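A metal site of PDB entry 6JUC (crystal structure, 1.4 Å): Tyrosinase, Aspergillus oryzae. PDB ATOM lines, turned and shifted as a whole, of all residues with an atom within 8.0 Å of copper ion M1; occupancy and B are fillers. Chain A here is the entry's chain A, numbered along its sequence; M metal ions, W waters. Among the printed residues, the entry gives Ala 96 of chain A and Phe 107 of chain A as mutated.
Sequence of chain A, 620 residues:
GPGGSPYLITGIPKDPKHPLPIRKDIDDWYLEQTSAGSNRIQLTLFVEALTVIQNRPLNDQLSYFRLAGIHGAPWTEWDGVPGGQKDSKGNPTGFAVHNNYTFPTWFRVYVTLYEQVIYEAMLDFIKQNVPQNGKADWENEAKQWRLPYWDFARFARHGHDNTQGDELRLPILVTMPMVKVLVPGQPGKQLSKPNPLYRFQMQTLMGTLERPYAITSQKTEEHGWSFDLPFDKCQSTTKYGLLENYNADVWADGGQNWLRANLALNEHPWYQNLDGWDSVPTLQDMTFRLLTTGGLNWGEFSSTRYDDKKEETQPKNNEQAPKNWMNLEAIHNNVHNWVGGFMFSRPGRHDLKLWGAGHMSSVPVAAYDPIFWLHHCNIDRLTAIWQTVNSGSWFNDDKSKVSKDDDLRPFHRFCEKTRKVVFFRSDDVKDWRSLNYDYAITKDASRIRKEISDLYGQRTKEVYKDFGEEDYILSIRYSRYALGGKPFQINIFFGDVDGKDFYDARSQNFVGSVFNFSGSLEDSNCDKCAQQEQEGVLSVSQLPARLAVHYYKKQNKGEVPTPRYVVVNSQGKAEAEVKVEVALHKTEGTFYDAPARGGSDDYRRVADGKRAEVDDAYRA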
ATOM      1  N   HIS A  71      -3.648  23.203   8.478  1.00  0.00           N
ATOM      2  CA  HIS A  71      -2.855  21.982   8.612  1.00  0.00           C
ATOM      3  C   HIS A  71      -1.565  22.038   7.818  1.00  0.00           C
ATOM      4  O   HIS A  71      -0.523  21.550   8.270  1.00  0.00           O
ATOM      5  CB  HIS A  71      -3.737  20.814   8.160  1.00  0.00           C
ATOM      6  CG  HIS A  71      -3.105  19.460   8.152  1.00  0.00           C
ATOM      7  ND1 HIS A  71      -2.630  18.896   6.997  1.00  0.00           N
ATOM      8  CD2 HIS A  71      -2.880  18.572   9.146  1.00  0.00           C
ATOM      9  CE1 HIS A  71      -2.118  17.697   7.271  1.00  0.00           C
ATOM     10  NE2 HIS A  71      -2.270  17.487   8.557  1.00  0.00           N
ATOM     11  N   ALA A  96       0.253  21.954  11.912  1.00  0.00           N
ATOM     12  CA  ALA A  96      -0.060  20.601  12.357  1.00  0.00           C
ATOM     13  C   ALA A  96       1.138  19.952  13.032  1.00  0.00           C
ATOM     14  O   ALA A  96       2.292  20.151  12.642  1.00  0.00           O
ATOM     15  CB  ALA A  96      -0.524  19.769  11.169  1.00  0.00           C
ATOM     16  N   VAL A  97       0.848  19.127  14.031  1.00  0.00           N
ATOM     17  CA  VAL A  97       1.855  18.309  14.692  1.00  0.00           C
ATOM     18  C   VAL A  97       1.868  16.902  14.102  1.00  0.00           C
ATOM     19  O   VAL A  97       0.847  16.207  14.220  1.00  0.00           O
ATOM     20  CB  VAL A  97       1.580  18.185  16.204  1.00  0.00           C
ATOM     21  CG1 VAL A  97       2.620  17.282  16.848  1.00  0.00           C
ATOM     22  CG2 VAL A  97       1.557  19.562  16.849  1.00  0.00           C
ATOM     23  N   HIS A  98       2.998  16.554  13.510  1.00  0.00           N
ATOM     24  CA  HIS A  98       3.252  15.175  13.102  1.00  0.00           C
ATOM     25  C   HIS A  98       4.535  14.651  13.733  1.00  0.00           C
ATOM     26  O   HIS A  98       5.483  15.410  13.972  1.00  0.00           O
ATOM     27  CB  HIS A  98       3.376  15.037  11.585  1.00  0.00           C
ATOM     28  CG  HIS A  98       2.197  15.575  10.836  1.00  0.00           C
ATOM     29  ND1 HIS A  98       2.231  16.772  10.156  1.00  0.00           N
ATOM     30  CD2 HIS A  98       0.947  15.093  10.660  1.00  0.00           C
ATOM     31  CE1 HIS A  98       1.052  17.003   9.597  1.00  0.00           C
ATOM     32  NE2 HIS A  98       0.248  15.991   9.895  1.00  0.00           N
ATOM     33  N   PHE A 103       0.606  14.895  18.797  1.00  0.00           N
ATOM     34  CA  PHE A 103      -0.225  14.587  17.628  1.00  0.00           C
ATOM     35  C   PHE A 103      -1.682  14.407  18.018  1.00  0.00           C
ATOM     36  O   PHE A 103      -2.570  15.068  17.448  1.00  0.00           O
ATOM     37  CB  PHE A 103       0.333  13.371  16.888  1.00  0.00           C
ATOM     38  CG  PHE A 103      -0.602  12.727  15.909  1.00  0.00           C
ATOM     39  CD1 PHE A 103      -0.781  13.255  14.637  1.00  0.00           C
ATOM     40  CD2 PHE A 103      -1.317  11.593  16.270  1.00  0.00           C
ATOM     41  CE1 PHE A 103      -1.656  12.655  13.751  1.00  0.00           C
ATOM     42  CE2 PHE A 103      -2.202  11.003  15.382  1.00  0.00           C
ATOM     43  CZ  PHE A 103      -2.388  11.537  14.121  1.00  0.00           C
ATOM     44  N   PHE A 107      -4.595  17.528  17.173  1.00  0.00           N
ATOM     45  CA  PHE A 107      -5.729  17.219  16.295  1.00  0.00           C
ATOM     46  C   PHE A 107      -7.052  17.234  17.050  1.00  0.00           C
ATOM     47  O   PHE A 107      -8.094  17.528  16.439  1.00  0.00           O
ATOM     48  CB  PHE A 107      -5.544  15.875  15.574  1.00  0.00           C
ATOM     49  CG  PHE A 107      -4.655  16.068  14.362  1.00  0.00           C
ATOM     50  CD1 PHE A 107      -5.183  16.586  13.187  1.00  0.00           C
ATOM     51  CD2 PHE A 107      -3.293  15.783  14.398  1.00  0.00           C
ATOM     52  CE1 PHE A 107      -4.388  16.840  12.094  1.00  0.00           C
ATOM     53  CE2 PHE A 107      -2.490  16.037  13.310  1.00  0.00           C
ATOM     54  CZ  PHE A 107      -3.027  16.595  12.171  1.00  0.00           C
ATOM     55  N   TYR A 110      -8.094  20.703  16.684  1.00  0.00           N
ATOM     56  CA  TYR A 110      -8.383  20.997  15.281  1.00  0.00           C
ATOM     57  C   TYR A 110      -9.754  20.456  14.856  1.00  0.00           C
ATOM     58  O   TYR A 110     -10.509  21.169  14.201  1.00  0.00           O
ATOM     59  CB  TYR A 110      -7.326  20.367  14.398  1.00  0.00           C
ATOM     60  CG  TYR A 110      -7.222  20.865  12.983  1.00  0.00           C
ATOM     61  CD1 TYR A 110      -7.584  22.132  12.556  1.00  0.00           C
ATOM     62  CD2 TYR A 110      -6.688  19.962  12.054  1.00  0.00           C
ATOM     63  CE1 TYR A 110      -7.434  22.485  11.218  1.00  0.00           C
ATOM     64  CE2 TYR A 110      -6.517  20.312  10.740  1.00  0.00           C
ATOM     65  CZ  TYR A 110      -6.903  21.577  10.334  1.00  0.00           C
ATOM     66  OH  TYR A 110      -6.723  21.903   9.003  1.00  0.00           O
ATOM     67  N   GLU A 329      -0.615   7.060  15.411  1.00  0.00           N
ATOM     68  CA  GLU A 329      -0.237   7.884  14.265  1.00  0.00           C
ATOM     69  C   GLU A 329       0.117   7.040  13.053  1.00  0.00           C
ATOM     70  O   GLU A 329      -0.218   7.382  11.904  1.00  0.00           O
ATOM     71  CB  GLU A 329       0.945   8.795  14.661  1.00  0.00           C
ATOM     72  CG  GLU A 329       1.203   9.891  13.661  1.00  0.00           C
ATOM     73  CD  GLU A 329       2.263  10.889  14.046  1.00  0.00           C
ATOM     74  OE1 GLU A 329       2.819  10.769  15.162  1.00  0.00           O
ATOM     75  OE2 GLU A 329       2.514  11.818  13.231  1.00  0.00           O
ATOM     76  N   HIS A 332      -2.933   5.856  11.452  1.00  0.00           N
ATOM     77  CA  HIS A 332      -3.510   7.047  10.838  1.00  0.00           C
ATOM     78  C   HIS A 332      -2.803   7.368   9.523  1.00  0.00           C
ATOM     79  O   HIS A 332      -3.443   7.799   8.553  1.00  0.00           O
ATOM     80  CB  HIS A 332      -3.436   8.214  11.825  1.00  0.00           C
ATOM     81  CG  HIS A 332      -3.135   9.556  11.244  1.00  0.00           C
ATOM     82  ND1 HIS A 332      -1.861   9.921  10.873  1.00  0.00           N
ATOM     83  CD2 HIS A 332      -3.911  10.630  10.981  1.00  0.00           C
ATOM     84  CE1 HIS A 332      -1.876  11.152  10.390  1.00  0.00           C
ATOM     85  NE2 HIS A 332      -3.112  11.618  10.459  1.00  0.00           N
ATOM     86  N   ASN A 333      -1.501   7.163   9.445  1.00  0.00           N
ATOM     87  CA  ASN A 333      -0.697   7.417   8.258  1.00  0.00           C
ATOM     88  C   ASN A 333      -1.048   6.457   7.133  1.00  0.00           C
ATOM     89  O   ASN A 333      -1.158   6.875   5.978  1.00  0.00           O
ATOM     90  CB  ASN A 333       0.794   7.270   8.568  1.00  0.00           C
ATOM     91  CG  ASN A 333       1.349   8.390   9.412  1.00  0.00           C
ATOM     92  OD1 ASN A 333       0.685   9.410   9.643  1.00  0.00           O
ATOM     93  ND2 ASN A 333       2.566   8.172   9.887  1.00  0.00           N
ATOM     94  N   VAL A 335      -3.882   5.001   6.727  1.00  0.00           N
ATOM     95  CA  VAL A 335      -5.235   5.297   6.266  1.00  0.00           C
ATOM     96  C   VAL A 335      -5.212   6.475   5.310  1.00  0.00           C
ATOM     97  O   VAL A 335      -5.875   6.474   4.276  1.00  0.00           O
ATOM     98  CB  VAL A 335      -6.209   5.551   7.434  1.00  0.00           C
ATOM     99  CG1 VAL A 335      -7.545   6.082   6.948  1.00  0.00           C
ATOM    100  CG2 VAL A 335      -6.389   4.260   8.222  1.00  0.00           C
ATOM    101  N   HIS A 336      -4.369   7.477   5.592  1.00  0.00           N
ATOM    102  CA  HIS A 336      -4.215   8.574   4.629  1.00  0.00           C
ATOM    103  C   HIS A 336      -3.846   8.055   3.243  1.00  0.00           C
ATOM    104  O   HIS A 336      -4.420   8.441   2.220  1.00  0.00           O
ATOM    105  CB  HIS A 336      -3.136   9.508   5.159  1.00  0.00           C
ATOM    106  CG  HIS A 336      -3.639  10.648   5.999  1.00  0.00           C
ATOM    107  ND1 HIS A 336      -4.242  11.746   5.428  1.00  0.00           N
ATOM    108  CD2 HIS A 336      -3.619  10.891   7.337  1.00  0.00           C
ATOM    109  CE1 HIS A 336      -4.563  12.610   6.370  1.00  0.00           C
ATOM    110  NE2 HIS A 336      -4.213  12.121   7.551  1.00  0.00           N
ATOM    111  N   MET A 360      -5.491  12.903  -0.011  1.00  0.00           N
ATOM    112  CA  MET A 360      -5.376  12.377   1.348  1.00  0.00           C
ATOM    113  C   MET A 360      -4.027  11.743   1.635  1.00  0.00           C
ATOM    114  O   MET A 360      -3.660  11.575   2.792  1.00  0.00           O
ATOM    115  CB  MET A 360      -6.495  11.387   1.665  1.00  0.00           C
ATOM    116  CG  MET A 360      -7.740  12.083   2.202  1.00  0.00           C
ATOM    117  SD  MET A 360      -7.547  12.649   3.896  1.00  0.00           S
ATOM    118  CE  MET A 360      -7.701  11.099   4.774  1.00  0.00           C
ATOM    119  N   VAL A 363       0.662  15.250   2.888  1.00  0.00           N
ATOM    120  CA  VAL A 363       0.555  16.111   4.057  1.00  0.00           C
ATOM    121  C   VAL A 363       0.137  17.531   3.687  1.00  0.00           C
ATOM    122  O   VAL A 363      -0.805  18.074   4.277  1.00  0.00           O
ATOM    123  CB  VAL A 363       1.863  16.174   4.870  1.00  0.00           C
ATOM    124  CG1 VAL A 363       1.737  17.178   6.014  1.00  0.00           C
ATOM    125  CG2 VAL A 363       2.268  14.812   5.419  1.00  0.00           C
ATOM    126  N   ALA A 366      -3.740  17.186   2.352  1.00  0.00           N
ATOM    127  CA  ALA A 366      -4.750  16.197   2.760  1.00  0.00           C
ATOM    128  C   ALA A 366      -5.967  16.843   3.404  1.00  0.00           C
ATOM    129  O   ALA A 366      -7.089  16.346   3.247  1.00  0.00           O
ATOM    130  CB  ALA A 366      -4.149  15.153   3.688  1.00  0.00           C
ATOM    131  N   ALA A 367      -5.798  17.950   4.134  1.00  0.00           N
ATOM    132  CA  ALA A 367      -6.912  18.523   4.896  1.00  0.00           C
ATOM    133  C   ALA A 367      -8.023  19.048   3.995  1.00  0.00           C
ATOM    134  O   ALA A 367      -9.157  19.236   4.454  1.00  0.00           O
ATOM    135  CB  ALA A 367      -6.411  19.621   5.811  1.00  0.00           C
ATOM    136  N   PHE A 372     -10.924  13.933   5.398  1.00  0.00           N
ATOM    137  CA  PHE A 372      -9.840  14.152   6.356  1.00  0.00           C
ATOM    138  C   PHE A 372     -10.379  14.343   7.770  1.00  0.00           C
ATOM    139  O   PHE A 372      -9.870  13.781   8.741  1.00  0.00           O
ATOM    140  CB  PHE A 372      -9.091  15.397   5.902  1.00  0.00           C
ATOM    141  CG  PHE A 372      -8.074  15.936   6.860  1.00  0.00           C
ATOM    142  CD1 PHE A 372      -8.400  16.891   7.812  1.00  0.00           C
ATOM    143  CD2 PHE A 372      -6.759  15.461   6.797  1.00  0.00           C
ATOM    144  CE1 PHE A 372      -7.421  17.395   8.657  1.00  0.00           C
ATOM    145  CE2 PHE A 372      -5.785  15.978   7.631  1.00  0.00           C
ATOM    146  CZ  PHE A 372      -6.124  16.920   8.584  1.00  0.00           C
ATOM    147  N   TRP A 373     -11.441  15.157   7.883  1.00  0.00           N
ATOM    148  CA  TRP A 373     -11.960  15.557   9.189  1.00  0.00           C
ATOM    149  C   TRP A 373     -12.606  14.357   9.861  1.00  0.00           C
ATOM    150  O   TRP A 373     -12.604  14.217  11.084  1.00  0.00           O
ATOM    151  CB  TRP A 373     -12.976  16.692   8.996  1.00  0.00           C
ATOM    152  CG  TRP A 373     -12.349  17.816   8.217  1.00  0.00           C
ATOM    153  CD1 TRP A 373     -12.436  17.971   6.863  1.00  0.00           C
ATOM    154  CD2 TRP A 373     -11.539  18.893   8.711  1.00  0.00           C
ATOM    155  NE1 TRP A 373     -11.731  19.099   6.481  1.00  0.00           N
ATOM    156  CE2 TRP A 373     -11.173  19.681   7.605  1.00  0.00           C
ATOM    157  CE3 TRP A 373     -11.101  19.263   9.994  1.00  0.00           C
ATOM    158  CZ2 TRP A 373     -10.387  20.831   7.730  1.00  0.00           C
ATOM    159  CZ3 TRP A 373     -10.322  20.403  10.110  1.00  0.00           C
ATOM    160  CH2 TRP A 373      -9.973  21.160   8.993  1.00  0.00           C
ATOM    161  N   HIS A 375     -11.875  11.087   9.268  1.00  0.00           N
ATOM    162  CA  HIS A 375     -10.730  10.301   9.677  1.00  0.00           C
ATOM    163  C   HIS A 375     -10.196  10.777  11.014  1.00  0.00           C
ATOM    164  O   HIS A 375     -10.043  10.025  11.975  1.00  0.00           O
ATOM    165  CB  HIS A 375      -9.663  10.431   8.595  1.00  0.00           C
ATOM    166  CG  HIS A 375      -8.419   9.650   8.879  1.00  0.00           C
ATOM    167  ND1 HIS A 375      -8.416   8.419   9.518  1.00  0.00           N
ATOM    168  CD2 HIS A 375      -7.130   9.937   8.559  1.00  0.00           C
ATOM    169  CE1 HIS A 375      -7.160   7.997   9.592  1.00  0.00           C
ATOM    170  NE2 HIS A 375      -6.369   8.891   9.023  1.00  0.00           N
ATOM    171  N   HIS A 376      -9.910  12.088  11.083  1.00  0.00           N
ATOM    172  CA  HIS A 376      -9.381  12.641  12.313  1.00  0.00           C
ATOM    173  C   HIS A 376     -10.393  12.570  13.441  1.00  0.00           C
ATOM    174  O   HIS A 376     -10.010  12.428  14.593  1.00  0.00           O
ATOM    175  CB  HIS A 376      -8.843  14.068  12.098  1.00  0.00           C
ATOM    176  CG  HIS A 376      -7.389  13.923  11.689  1.00  0.00           C
ATOM    177  ND1 HIS A 376      -6.410  13.652  12.620  1.00  0.00           N
ATOM    178  CD2 HIS A 376      -6.799  13.919  10.486  1.00  0.00           C
ATOM    179  CE1 HIS A 376      -5.246  13.524  11.995  1.00  0.00           C
ATOM    180  NE2 HIS A 376      -5.458  13.692  10.695  1.00  0.00           N
ATOM    181  N   ILE A 379      -9.698   9.205  14.740  1.00  0.00           N
ATOM    182  CA  ILE A 379      -8.422   9.181  15.471  1.00  0.00           C
ATOM    183  C   ILE A 379      -8.616   9.775  16.857  1.00  0.00           C
ATOM    184  O   ILE A 379      -8.036   9.290  17.829  1.00  0.00           O
ATOM    185  CB  ILE A 379      -7.334   9.891  14.653  1.00  0.00           C
ATOM    186  CG1 ILE A 379      -6.994   9.186  13.332  1.00  0.00           C
ATOM    187  CG2 ILE A 379      -6.048  10.132  15.431  1.00  0.00           C
ATOM    188  CD1 ILE A 379      -6.489   7.751  13.536  1.00  0.00           C
ATOM    189  N   PHE A 517       3.923   9.232   5.798  1.00  0.00           N
ATOM    190  CA  PHE A 517       3.064  10.403   5.615  1.00  0.00           C
ATOM    191  C   PHE A 517       3.870  11.650   5.944  1.00  0.00           C
ATOM    192  O   PHE A 517       3.874  12.176   7.058  1.00  0.00           O
ATOM    193  CB  PHE A 517       1.840  10.293   6.513  1.00  0.00           C
ATOM    194  CG  PHE A 517       0.783  11.349   6.310  1.00  0.00           C
ATOM    195  CD1 PHE A 517       0.220  11.556   5.053  1.00  0.00           C
ATOM    196  CD2 PHE A 517       0.338  12.122   7.361  1.00  0.00           C
ATOM    197  CE1 PHE A 517      -0.779  12.495   4.848  1.00  0.00           C
ATOM    198  CE2 PHE A 517      -0.672  13.064   7.175  1.00  0.00           C
ATOM    199  CZ  PHE A 517      -1.235  13.239   5.917  1.00  0.00           C
HETATM  200 CU    CU M   1      -4.262  13.034   9.286  1.00  0.00          CU
HETATM  201 CU    CU M   2      -1.628  15.741   9.306  1.00  0.00          CU
HETATM  202  O   HOH W   1      -2.707  14.726   9.225  1.00  0.00           O
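The backbone carbonyl oxygen (O) of Glu 329 sits at hydrogen-bond distance from a ring nitrogen (ND1) of His 332 (3.2 Å). The backbone carbonyl oxygen (O) of Met 360 sits at hydrogen-bond distance from a ring nitrogen (ND1) of His 336 (2.7 Å). The side-chain amide oxygen (OD1) of Asn 333 sits at hydrogen-bond distance from a ring nitrogen (ND1) of His 332. NE2 of His 375 lies within hydrogen-bond range of O of His 332, at 3.2 Å.
Phe 372 touches copper ion M1.
Copper ion M1 is bound by NE2 of His 336, 2.0 Å away. NE2 of His 376 binds copper ion M1, 2.0 Å away. A ring nitrogen (NE2) of His 332 binds copper ion M1 (2.2 Å). Water W1 binds copper ion M1 (2.3 Å). Copper ion M1 has four donor atoms within binding distance.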
